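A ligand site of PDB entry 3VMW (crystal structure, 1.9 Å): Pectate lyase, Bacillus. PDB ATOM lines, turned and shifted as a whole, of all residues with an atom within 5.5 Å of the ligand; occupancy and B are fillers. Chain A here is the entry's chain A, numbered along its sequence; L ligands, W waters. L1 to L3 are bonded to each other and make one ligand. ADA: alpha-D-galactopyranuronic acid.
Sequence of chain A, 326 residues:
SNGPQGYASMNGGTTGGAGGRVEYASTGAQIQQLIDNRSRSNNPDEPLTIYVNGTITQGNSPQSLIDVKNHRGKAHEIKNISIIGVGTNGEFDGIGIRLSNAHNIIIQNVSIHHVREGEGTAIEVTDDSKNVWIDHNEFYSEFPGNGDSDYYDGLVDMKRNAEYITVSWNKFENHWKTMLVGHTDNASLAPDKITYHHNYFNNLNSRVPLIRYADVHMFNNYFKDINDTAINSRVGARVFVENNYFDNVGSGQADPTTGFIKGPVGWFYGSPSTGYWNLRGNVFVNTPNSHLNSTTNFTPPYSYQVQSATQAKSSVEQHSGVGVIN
An oxygen (O6B) of ADA L1 is in salt-bridge range of the side-chain amino group (NZ) of Lys 262, 2.9 Å away. An oxygen (O6A) of ADA L3 lies within salt-bridge range of the guanidinium group (NH2) of Arg 234. An oxygen (O6B) of ADA L2 sits at hydrogen-bond distance from the side-chain hydroxyl (OG) of Ser 206, at 2.8 Å. NH2 of Arg 207 lies within hydrogen-bond range of O4 of ADA L3 (3.0 Å).
Water W4 bridges an oxygen (O6A) of ADA L2 (2.6 Å) and the side-chain hydroxyl of Ser 149 (2.7 Å). Water W7 lies within hydrogen-bond range of an oxygen (O6A) of ADA L2 (2.7 Å), the side-chain hydroxyl of Ser 206 (2.7 Å), the side-chain amide oxygen of Asn 205 (2.9 Å) and the backbone carbonyl oxygen of Trp 176 (3.3 Å). Water W6 lies within hydrogen-bond range of the backbone carbonyl oxygen (O) of Tyr 269 (2.7 Å), an oxygen (O3) of ADA L2 (2.8 Å) and the side-chain hydroxyl (OG1) of Thr 257 (3.4 Å). Water W3 lies within hydrogen-bond range of O6A of ADA L3 (2.8 Å) and NE of Arg 207 (2.9 Å). Water W5 lies within hydrogen-bond range of OD2 of Asp 255 (2.7 Å), OG1 of Thr 257 (2.8 Å) and O6B of ADA L1 (2.9 Å). Water W8 bridges the guanidinium group (NH1) of Arg 212 and an oxygen (O4) of ADA L3.
The side-chain amino group (NZ) of Lys 262 is in salt-bridge range of the side-chain carboxylate (OD2) of Asp 228. NE of Arg 234 sits at hydrogen-bond distance from O of Gly 270 (3.4 Å). The side-chain amide nitrogen of Asn 232 lies close to the guanidinium group of Arg 234 (3.3 Å). The guanidinium group (NE) of Arg 234 sits at hydrogen-bond distance from the side-chain hydroxyl (OG) of Ser 271. O of Trp 176 lies within hydrogen-bond range of N of Ser 206 (3.0 Å). The side-chain carboxylate (OD2) of Asp 228 is in hydrogen-bond range of the side-chain hydroxyl (OH) of Tyr 269, at 2.5 Å. The backbone NH (N) of Asp 228 sits at hydrogen-bond distance from the backbone carbonyl oxygen (O) of Asn 205 (2.9 Å). The backbone NH (N) of Tyr 269 lies within hydrogen-bond range of the side-chain carboxylate (OD1) of Asp 255 (2.8 Å).
OD1 of Asn 205 touches O6A of ADA L2, at 3.9 Å. Leu 210 touches the ligand. OD1 of Asp 228 touches C1 of ADA L1, at 3.5 Å. Pro 256 touches the ligand. Tyr 269 touches the ligand. Hydrophobic or aromatic side chains that line the ligand: Leu 210, Pro 256 and Tyr 269. Nine residues have an atom within 4 Å of the ligand: Asn 205, Ser 206, Arg 207, Leu 210, Asp 228, Arg 234, Pro 256, Lys 262 and Tyr 269.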
ATOM      1  N   SER A 149      14.951  36.382  -5.952  1.00  0.00           N
ATOM      2  CA  SER A 149      14.624  35.083  -6.544  1.00  0.00           C
ATOM      3  C   SER A 149      13.231  35.064  -7.186  1.00  0.00           C
ATOM      4  O   SER A 149      12.936  34.237  -8.044  1.00  0.00           O
ATOM      5  CB  SER A 149      14.725  33.982  -5.486  1.00  0.00           C
ATOM      6  OG  SER A 149      13.725  34.136  -4.471  1.00  0.00           O
ATOM      7  N   ASP A 150      12.392  36.020  -6.771  1.00  0.00           N
ATOM      8  CA  ASP A 150      10.997  36.078  -7.231  1.00  0.00           C
ATOM      9  C   ASP A 150      10.751  37.122  -8.306  1.00  0.00           C
ATOM     10  O   ASP A 150       9.615  37.263  -8.788  1.00  0.00           O
ATOM     11  CB  ASP A 150      10.059  36.378  -6.048  1.00  0.00           C
ATOM     12  CG  ASP A 150      10.130  35.326  -4.968  1.00  0.00           C
ATOM     13  OD1 ASP A 150      10.258  34.108  -5.284  1.00  0.00           O
ATOM     14  OD2 ASP A 150      10.057  35.736  -3.786  1.00  0.00           O
ATOM     15  N   TRP A 176      16.912  31.758 -11.086  1.00  0.00           N
ATOM     16  CA  TRP A 176      16.690  31.276  -9.716  1.00  0.00           C
ATOM     17  C   TRP A 176      15.801  30.020  -9.617  1.00  0.00           C
ATOM     18  O   TRP A 176      16.299  28.931  -9.376  1.00  0.00           O
ATOM     19  CB  TRP A 176      16.096  32.393  -8.835  1.00  0.00           C
ATOM     20  CG  TRP A 176      17.055  33.492  -8.548  1.00  0.00           C
ATOM     21  CD1 TRP A 176      17.370  34.553  -9.362  1.00  0.00           C
ATOM     22  CD2 TRP A 176      17.834  33.665  -7.340  1.00  0.00           C
ATOM     23  NE1 TRP A 176      18.305  35.366  -8.734  1.00  0.00           N
ATOM     24  CE2 TRP A 176      18.601  34.845  -7.507  1.00  0.00           C
ATOM     25  CE3 TRP A 176      17.952  32.950  -6.136  1.00  0.00           C
ATOM     26  CZ2 TRP A 176      19.471  35.335  -6.500  1.00  0.00           C
ATOM     27  CZ3 TRP A 176      18.821  33.414  -5.155  1.00  0.00           C
ATOM     28  CH2 TRP A 176      19.572  34.589  -5.356  1.00  0.00           C
ATOM     29  N   LYS A 177      14.483  30.191  -9.768  1.00  0.00           N
ATOM     30  CA  LYS A 177      13.514  29.135  -9.517  1.00  0.00           C
ATOM     31  C   LYS A 177      13.177  28.405 -10.813  1.00  0.00           C
ATOM     32  O   LYS A 177      12.251  28.783 -11.513  1.00  0.00           O
ATOM     33  CB  LYS A 177      12.218  29.722  -8.927  1.00  0.00           C
ATOM     34  CG  LYS A 177      12.480  30.459  -7.608  1.00  0.00           C
ATOM     35  CD  LYS A 177      11.178  30.929  -6.974  1.00  0.00           C
ATOM     36  CE  LYS A 177      10.402  31.880  -7.893  1.00  0.00           C
ATOM     37  NZ  LYS A 177       9.153  32.336  -7.199  1.00  0.00           N
ATOM     38  N   ASN A 205      19.789  28.481  -9.432  1.00  0.00           N
ATOM     39  CA  ASN A 205      19.803  28.381  -7.975  1.00  0.00           C
ATOM     40  C   ASN A 205      19.150  27.112  -7.454  1.00  0.00           C
ATOM     41  O   ASN A 205      19.748  26.393  -6.644  1.00  0.00           O
ATOM     42  CB  ASN A 205      19.144  29.595  -7.316  1.00  0.00           C
ATOM     43  CG  ASN A 205      19.346  29.622  -5.817  1.00  0.00           C
ATOM     44  OD1 ASN A 205      18.381  29.685  -5.046  1.00  0.00           O
ATOM     45  ND2 ASN A 205      20.591  29.585  -5.399  1.00  0.00           N
ATOM     46  N   SER A 206      17.909  26.855  -7.891  1.00  0.00           N
ATOM     47  CA  SER A 206      17.165  25.744  -7.343  1.00  0.00           C
ATOM     48  C   SER A 206      16.066  25.273  -8.303  1.00  0.00           C
ATOM     49  O   SER A 206      15.873  25.815  -9.394  1.00  0.00           O
ATOM     50  CB  SER A 206      16.532  26.157  -5.980  1.00  0.00           C
ATOM     51  OG  SER A 206      15.477  27.102  -6.214  1.00  0.00           O
ATOM     52  N   ARG A 207      15.361  24.248  -7.859  1.00  0.00           N
ATOM     53  CA  ARG A 207      14.220  23.678  -8.560  1.00  0.00           C
ATOM     54  C   ARG A 207      14.588  23.039  -9.883  1.00  0.00           C
ATOM     55  O   ARG A 207      14.153  23.522 -10.943  1.00  0.00           O
ATOM     56  CB  ARG A 207      13.112  24.735  -8.777  1.00  0.00           C
ATOM     57  CG  ARG A 207      12.594  25.306  -7.464  1.00  0.00           C
ATOM     58  CD  ARG A 207      11.327  26.172  -7.744  1.00  0.00           C
ATOM     59  NE  ARG A 207      10.778  26.718  -6.517  1.00  0.00           N
ATOM     60  CZ  ARG A 207       9.652  27.420  -6.479  1.00  0.00           C
ATOM     61  NH1 ARG A 207       9.017  27.685  -7.617  1.00  0.00           N
ATOM     62  NH2 ARG A 207       9.170  27.865  -5.325  1.00  0.00           N
ATOM     63  N   LEU A 210      11.710  21.120  -8.907  1.00  0.00           N
ATOM     64  CA  LEU A 210      10.986  20.892  -7.656  1.00  0.00           C
ATOM     65  C   LEU A 210       9.816  19.956  -7.999  1.00  0.00           C
ATOM     66  O   LEU A 210       8.904  20.343  -8.756  1.00  0.00           O
ATOM     67  CB  LEU A 210      10.450  22.210  -7.147  1.00  0.00           C
ATOM     68  CG  LEU A 210       9.752  22.275  -5.757  1.00  0.00           C
ATOM     69  CD1 LEU A 210       9.380  23.731  -5.414  1.00  0.00           C
ATOM     70  CD2 LEU A 210       8.506  21.447  -5.766  1.00  0.00           C
ATOM     71  N   ARG A 212       6.603  17.681  -6.722  1.00  0.00           N
ATOM     72  CA  ARG A 212       5.636  17.180  -5.730  1.00  0.00           C
ATOM     73  C   ARG A 212       4.785  16.086  -6.379  1.00  0.00           C
ATOM     74  O   ARG A 212       4.318  16.267  -7.512  1.00  0.00           O
ATOM     75  CB  ARG A 212       4.692  18.313  -5.285  1.00  0.00           C
ATOM     76  CG  ARG A 212       5.354  19.505  -4.582  1.00  0.00           C
ATOM     77  CD  ARG A 212       4.229  20.511  -4.229  1.00  0.00           C
ATOM     78  NE  ARG A 212       4.596  21.530  -3.250  1.00  0.00           N
ATOM     79  CZ  ARG A 212       5.141  22.708  -3.537  1.00  0.00           C
ATOM     80  NH1 ARG A 212       5.413  23.038  -4.791  1.00  0.00           N
ATOM     81  NH2 ARG A 212       5.387  23.565  -2.533  1.00  0.00           N
ATOM     82  N   ASP A 228      22.232  26.085  -5.212  1.00  0.00           N
ATOM     83  CA  ASP A 228      21.681  25.615  -3.927  1.00  0.00           C
ATOM     84  C   ASP A 228      21.318  24.142  -3.951  1.00  0.00           C
ATOM     85  O   ASP A 228      21.988  23.348  -3.281  1.00  0.00           O
ATOM     86  CB  ASP A 228      20.489  26.474  -3.484  1.00  0.00           C
ATOM     87  CG  ASP A 228      20.350  26.525  -1.978  1.00  0.00           C
ATOM     88  OD1 ASP A 228      21.321  26.874  -1.294  1.00  0.00           O
ATOM     89  OD2 ASP A 228      19.269  26.176  -1.480  1.00  0.00           O
ATOM     90  N   ASN A 232      14.544  18.086  -6.307  1.00  0.00           N
ATOM     91  CA  ASN A 232      13.913  18.118  -4.999  1.00  0.00           C
ATOM     92  C   ASN A 232      12.646  17.278  -5.056  1.00  0.00           C
ATOM     93  O   ASN A 232      11.693  17.665  -5.720  1.00  0.00           O
ATOM     94  CB  ASN A 232      13.556  19.569  -4.650  1.00  0.00           C
ATOM     95  CG  ASN A 232      13.041  19.703  -3.212  1.00  0.00           C
ATOM     96  OD1 ASN A 232      12.894  18.699  -2.515  1.00  0.00           O
ATOM     97  ND2 ASN A 232      12.766  20.948  -2.763  1.00  0.00           N
ATOM     98  N   ARG A 234       9.463  15.577  -3.372  1.00  0.00           N
ATOM     99  CA  ARG A 234       8.623  15.872  -2.206  1.00  0.00           C
ATOM    100  C   ARG A 234       7.297  15.132  -2.241  1.00  0.00           C
ATOM    101  O   ARG A 234       6.813  14.738  -3.318  1.00  0.00           O
ATOM    102  CB  ARG A 234       8.335  17.385  -2.180  1.00  0.00           C
ATOM    103  CG  ARG A 234       9.561  18.217  -1.837  1.00  0.00           C
ATOM    104  CD  ARG A 234       9.480  19.606  -2.454  1.00  0.00           C
ATOM    105  NE  ARG A 234       8.638  20.520  -1.665  1.00  0.00           N
ATOM    106  CZ  ARG A 234       8.867  21.833  -1.553  1.00  0.00           C
ATOM    107  NH1 ARG A 234       8.079  22.586  -0.795  1.00  0.00           N
ATOM    108  NH2 ARG A 234       9.902  22.387  -2.208  1.00  0.00           N
ATOM    109  N   ASP A 255      20.235  21.354   4.805  1.00  0.00           N
ATOM    110  CA  ASP A 255      18.994  22.109   4.657  1.00  0.00           C
ATOM    111  C   ASP A 255      18.426  22.416   6.050  1.00  0.00           C
ATOM    112  O   ASP A 255      18.253  21.513   6.889  1.00  0.00           O
ATOM    113  CB  ASP A 255      18.015  21.283   3.812  1.00  0.00           C
ATOM    114  CG  ASP A 255      16.723  22.047   3.472  1.00  0.00           C
ATOM    115  OD1 ASP A 255      16.440  22.256   2.260  1.00  0.00           O
ATOM    116  OD2 ASP A 255      15.983  22.376   4.409  1.00  0.00           O
ATOM    117  N   PRO A 256      18.149  23.701   6.324  1.00  0.00           N
ATOM    118  CA  PRO A 256      17.711  24.064   7.679  1.00  0.00           C
ATOM    119  C   PRO A 256      16.299  23.590   7.985  1.00  0.00           C
ATOM    120  O   PRO A 256      15.884  23.640   9.143  1.00  0.00           O
ATOM    121  CB  PRO A 256      17.809  25.595   7.698  1.00  0.00           C
ATOM    122  CG  PRO A 256      17.698  25.992   6.264  1.00  0.00           C
ATOM    123  CD  PRO A 256      18.335  24.887   5.459  1.00  0.00           C
ATOM    124  N   THR A 257      15.573  23.130   6.969  1.00  0.00           N
ATOM    125  CA  THR A 257      14.233  22.609   7.219  1.00  0.00           C
ATOM    126  C   THR A 257      14.201  21.073   7.286  1.00  0.00           C
ATOM    127  O   THR A 257      13.692  20.506   8.241  1.00  0.00           O
ATOM    128  CB  THR A 257      13.264  23.091   6.132  1.00  0.00           C
ATOM    129  OG1 THR A 257      13.275  24.524   6.132  1.00  0.00           O
ATOM    130  CG2 THR A 257      11.851  22.573   6.414  1.00  0.00           C
ATOM    131  N   LYS A 262      22.391  19.604   0.900  1.00  0.00           N
ATOM    132  CA  LYS A 262      21.995  20.208  -0.350  1.00  0.00           C
ATOM    133  C   LYS A 262      22.893  19.793  -1.514  1.00  0.00           C
ATOM    134  O   LYS A 262      24.101  20.058  -1.531  1.00  0.00           O
ATOM    135  CB  LYS A 262      21.919  21.740  -0.216  1.00  0.00           C
ATOM    136  CG  LYS A 262      20.701  22.176   0.622  1.00  0.00           C
ATOM    137  CD  LYS A 262      20.662  23.708   0.758  1.00  0.00           C
ATOM    138  CE  LYS A 262      19.358  24.163   1.407  1.00  0.00           C
ATOM    139  NZ  LYS A 262      19.268  25.642   1.411  1.00  0.00           N
ATOM    140  N   PHE A 268      14.153  18.973   0.103  1.00  0.00           N
ATOM    141  CA  PHE A 268      14.651  20.282   0.539  1.00  0.00           C
ATOM    142  C   PHE A 268      13.506  21.276   0.763  1.00  0.00           C
ATOM    143  O   PHE A 268      12.443  21.140   0.159  1.00  0.00           O
ATOM    144  CB  PHE A 268      15.624  20.856  -0.519  1.00  0.00           C
ATOM    145  CG  PHE A 268      16.689  19.894  -0.961  1.00  0.00           C
ATOM    146  CD1 PHE A 268      17.690  19.501  -0.091  1.00  0.00           C
ATOM    147  CD2 PHE A 268      16.702  19.395  -2.281  1.00  0.00           C
ATOM    148  CE1 PHE A 268      18.668  18.594  -0.504  1.00  0.00           C
ATOM    149  CE2 PHE A 268      17.680  18.506  -2.696  1.00  0.00           C
ATOM    150  CZ  PHE A 268      18.672  18.103  -1.805  1.00  0.00           C
ATOM    151  N   TYR A 269      13.728  22.256   1.641  1.00  0.00           N
ATOM    152  CA  TYR A 269      12.895  23.454   1.730  1.00  0.00           C
ATOM    153  C   TYR A 269      11.510  23.308   2.392  1.00  0.00           C
ATOM    154  O   TYR A 269      11.082  24.178   3.144  1.00  0.00           O
ATOM    155  CB  TYR A 269      12.661  24.013   0.345  1.00  0.00           C
ATOM    156  CG  TYR A 269      13.918  24.355  -0.399  1.00  0.00           C
ATOM    157  CD1 TYR A 269      15.026  24.916   0.235  1.00  0.00           C
ATOM    158  CD2 TYR A 269      13.996  24.124  -1.766  1.00  0.00           C
ATOM    159  CE1 TYR A 269      16.215  25.231  -0.517  1.00  0.00           C
ATOM    160  CE2 TYR A 269      15.138  24.413  -2.498  1.00  0.00           C
ATOM    161  CZ  TYR A 269      16.227  24.970  -1.883  1.00  0.00           C
ATOM    162  OH  TYR A 269      17.309  25.250  -2.674  1.00  0.00           O
ATOM    163  N   GLY A 270      10.787  22.239   2.084  1.00  0.00           N
ATOM    164  CA  GLY A 270       9.412  22.203   2.557  1.00  0.00           C
ATOM    165  C   GLY A 270       8.610  20.999   2.127  1.00  0.00           C
ATOM    166  O   GLY A 270       9.184  20.021   1.628  1.00  0.00           O
ATOM    167  N   SER A 271       7.292  21.109   2.338  1.00  0.00           N
ATOM    168  CA  SER A 271       6.338  20.011   2.237  1.00  0.00           C
ATOM    169  C   SER A 271       6.452  19.085   3.468  1.00  0.00           C
ATOM    170  O   SER A 271       7.525  18.921   4.047  1.00  0.00           O
ATOM    171  CB  SER A 271       6.477  19.239   0.913  1.00  0.00           C
ATOM    172  OG  SER A 271       6.303  20.121  -0.209  1.00  0.00           O
HETATM  173  C1  ADA L   1      19.646  28.914   0.990  1.00  0.00           C
HETATM  174  C2  ADA L   1      19.027  29.999   0.185  1.00  0.00           C
HETATM  175  C3  ADA L   1      18.017  30.758   0.934  1.00  0.00           C
HETATM  176  C4  ADA L   1      17.036  29.919   1.619  1.00  0.00           C
HETATM  177  C5  ADA L   1      17.722  28.836   2.397  1.00  0.00           C
HETATM  178  C6  ADA L   1      16.770  27.867   2.900  1.00  0.00           C
HETATM  179  O2  ADA L   1      20.102  30.825  -0.229  1.00  0.00           O
HETATM  180  O3  ADA L   1      17.371  31.713   0.065  1.00  0.00           O
HETATM  181  O4  ADA L   1      16.075  29.298   0.693  1.00  0.00           O
HETATM  182  O5  ADA L   1      18.651  28.109   1.593  1.00  0.00           O
HETATM  183  O6B ADA L   1      16.911  26.649   2.663  1.00  0.00           O
HETATM  184  O6A ADA L   1      15.789  28.291   3.531  1.00  0.00           O
HETATM  185  C1  ADA L   2      15.000  30.089   0.231  1.00  0.00           C
HETATM  186  C2  ADA L   2      13.714  29.611   0.874  1.00  0.00           C
HETATM  187  C3  ADA L   2      13.335  28.264   0.364  1.00  0.00           C
HETATM  188  C4  ADA L   2      13.192  28.264  -1.078  1.00  0.00           C
HETATM  189  C5  ADA L   2      14.496  28.679  -1.679  1.00  0.00           C
HETATM  190  C6  ADA L   2      14.463  28.740  -3.151  1.00  0.00           C
HETATM  191  O2  ADA L   2      13.854  29.623   2.277  1.00  0.00           O
HETATM  192  O3  ADA L   2      12.179  27.773   1.060  1.00  0.00           O
HETATM  193  O4  ADA L   2      12.141  29.192  -1.485  1.00  0.00           O
HETATM  194  O5  ADA L   2      14.905  30.020  -1.167  1.00  0.00           O
HETATM  195  O6B ADA L   2      14.202  27.738  -3.844  1.00  0.00           O
HETATM  196  O6A ADA L   2      14.729  29.841  -3.710  1.00  0.00           O
HETATM  197  C1  ADA L   3      11.346  28.871  -2.583  1.00  0.00           C
HETATM  198  C2  ADA L   3      10.170  29.833  -2.555  1.00  0.00           C
HETATM  199  C3  ADA L   3       9.242  29.531  -1.431  1.00  0.00           C
HETATM  200  C4  ADA L   3       8.789  28.159  -1.390  1.00  0.00           C
HETATM  201  C5  ADA L   3       9.962  27.193  -1.454  1.00  0.00           C
HETATM  202  C6  ADA L   3       9.617  25.780  -1.555  1.00  0.00           C
HETATM  203  O2  ADA L   3      10.736  31.096  -2.382  1.00  0.00           O
HETATM  204  O3  ADA L   3       8.089  30.414  -1.557  1.00  0.00           O
HETATM  205  O4  ADA L   3       7.953  27.947  -2.534  1.00  0.00           O
HETATM  206  O5  ADA L   3      10.912  27.527  -2.554  1.00  0.00           O
HETATM  207  O6B ADA L   3       8.752  25.280  -0.787  1.00  0.00           O
HETATM  208  O6A ADA L   3      10.240  25.021  -2.379  1.00  0.00           O
HETATM  209  O   HOH W   1       8.257  26.119   1.724  1.00  0.00           O
HETATM  210  O   HOH W   2      10.271  29.682   2.204  1.00  0.00           O
HETATM  211  O   HOH W   3      12.226  25.705  -4.174  1.00  0.00           O
HETATM  212  O   HOH W   4      13.407  31.967  -2.937  1.00  0.00           O
HETATM  213  O   HOH W   5      15.054  24.853   4.025  1.00  0.00           O
HETATM  214  O   HOH W   6      12.359  26.504   3.497  1.00  0.00           O
HETATM  215  O   HOH W   7      15.736  29.824  -6.248  1.00  0.00           O
HETATM  216  O   HOH W   8       6.063  26.018  -4.391  1.00  0.00           O
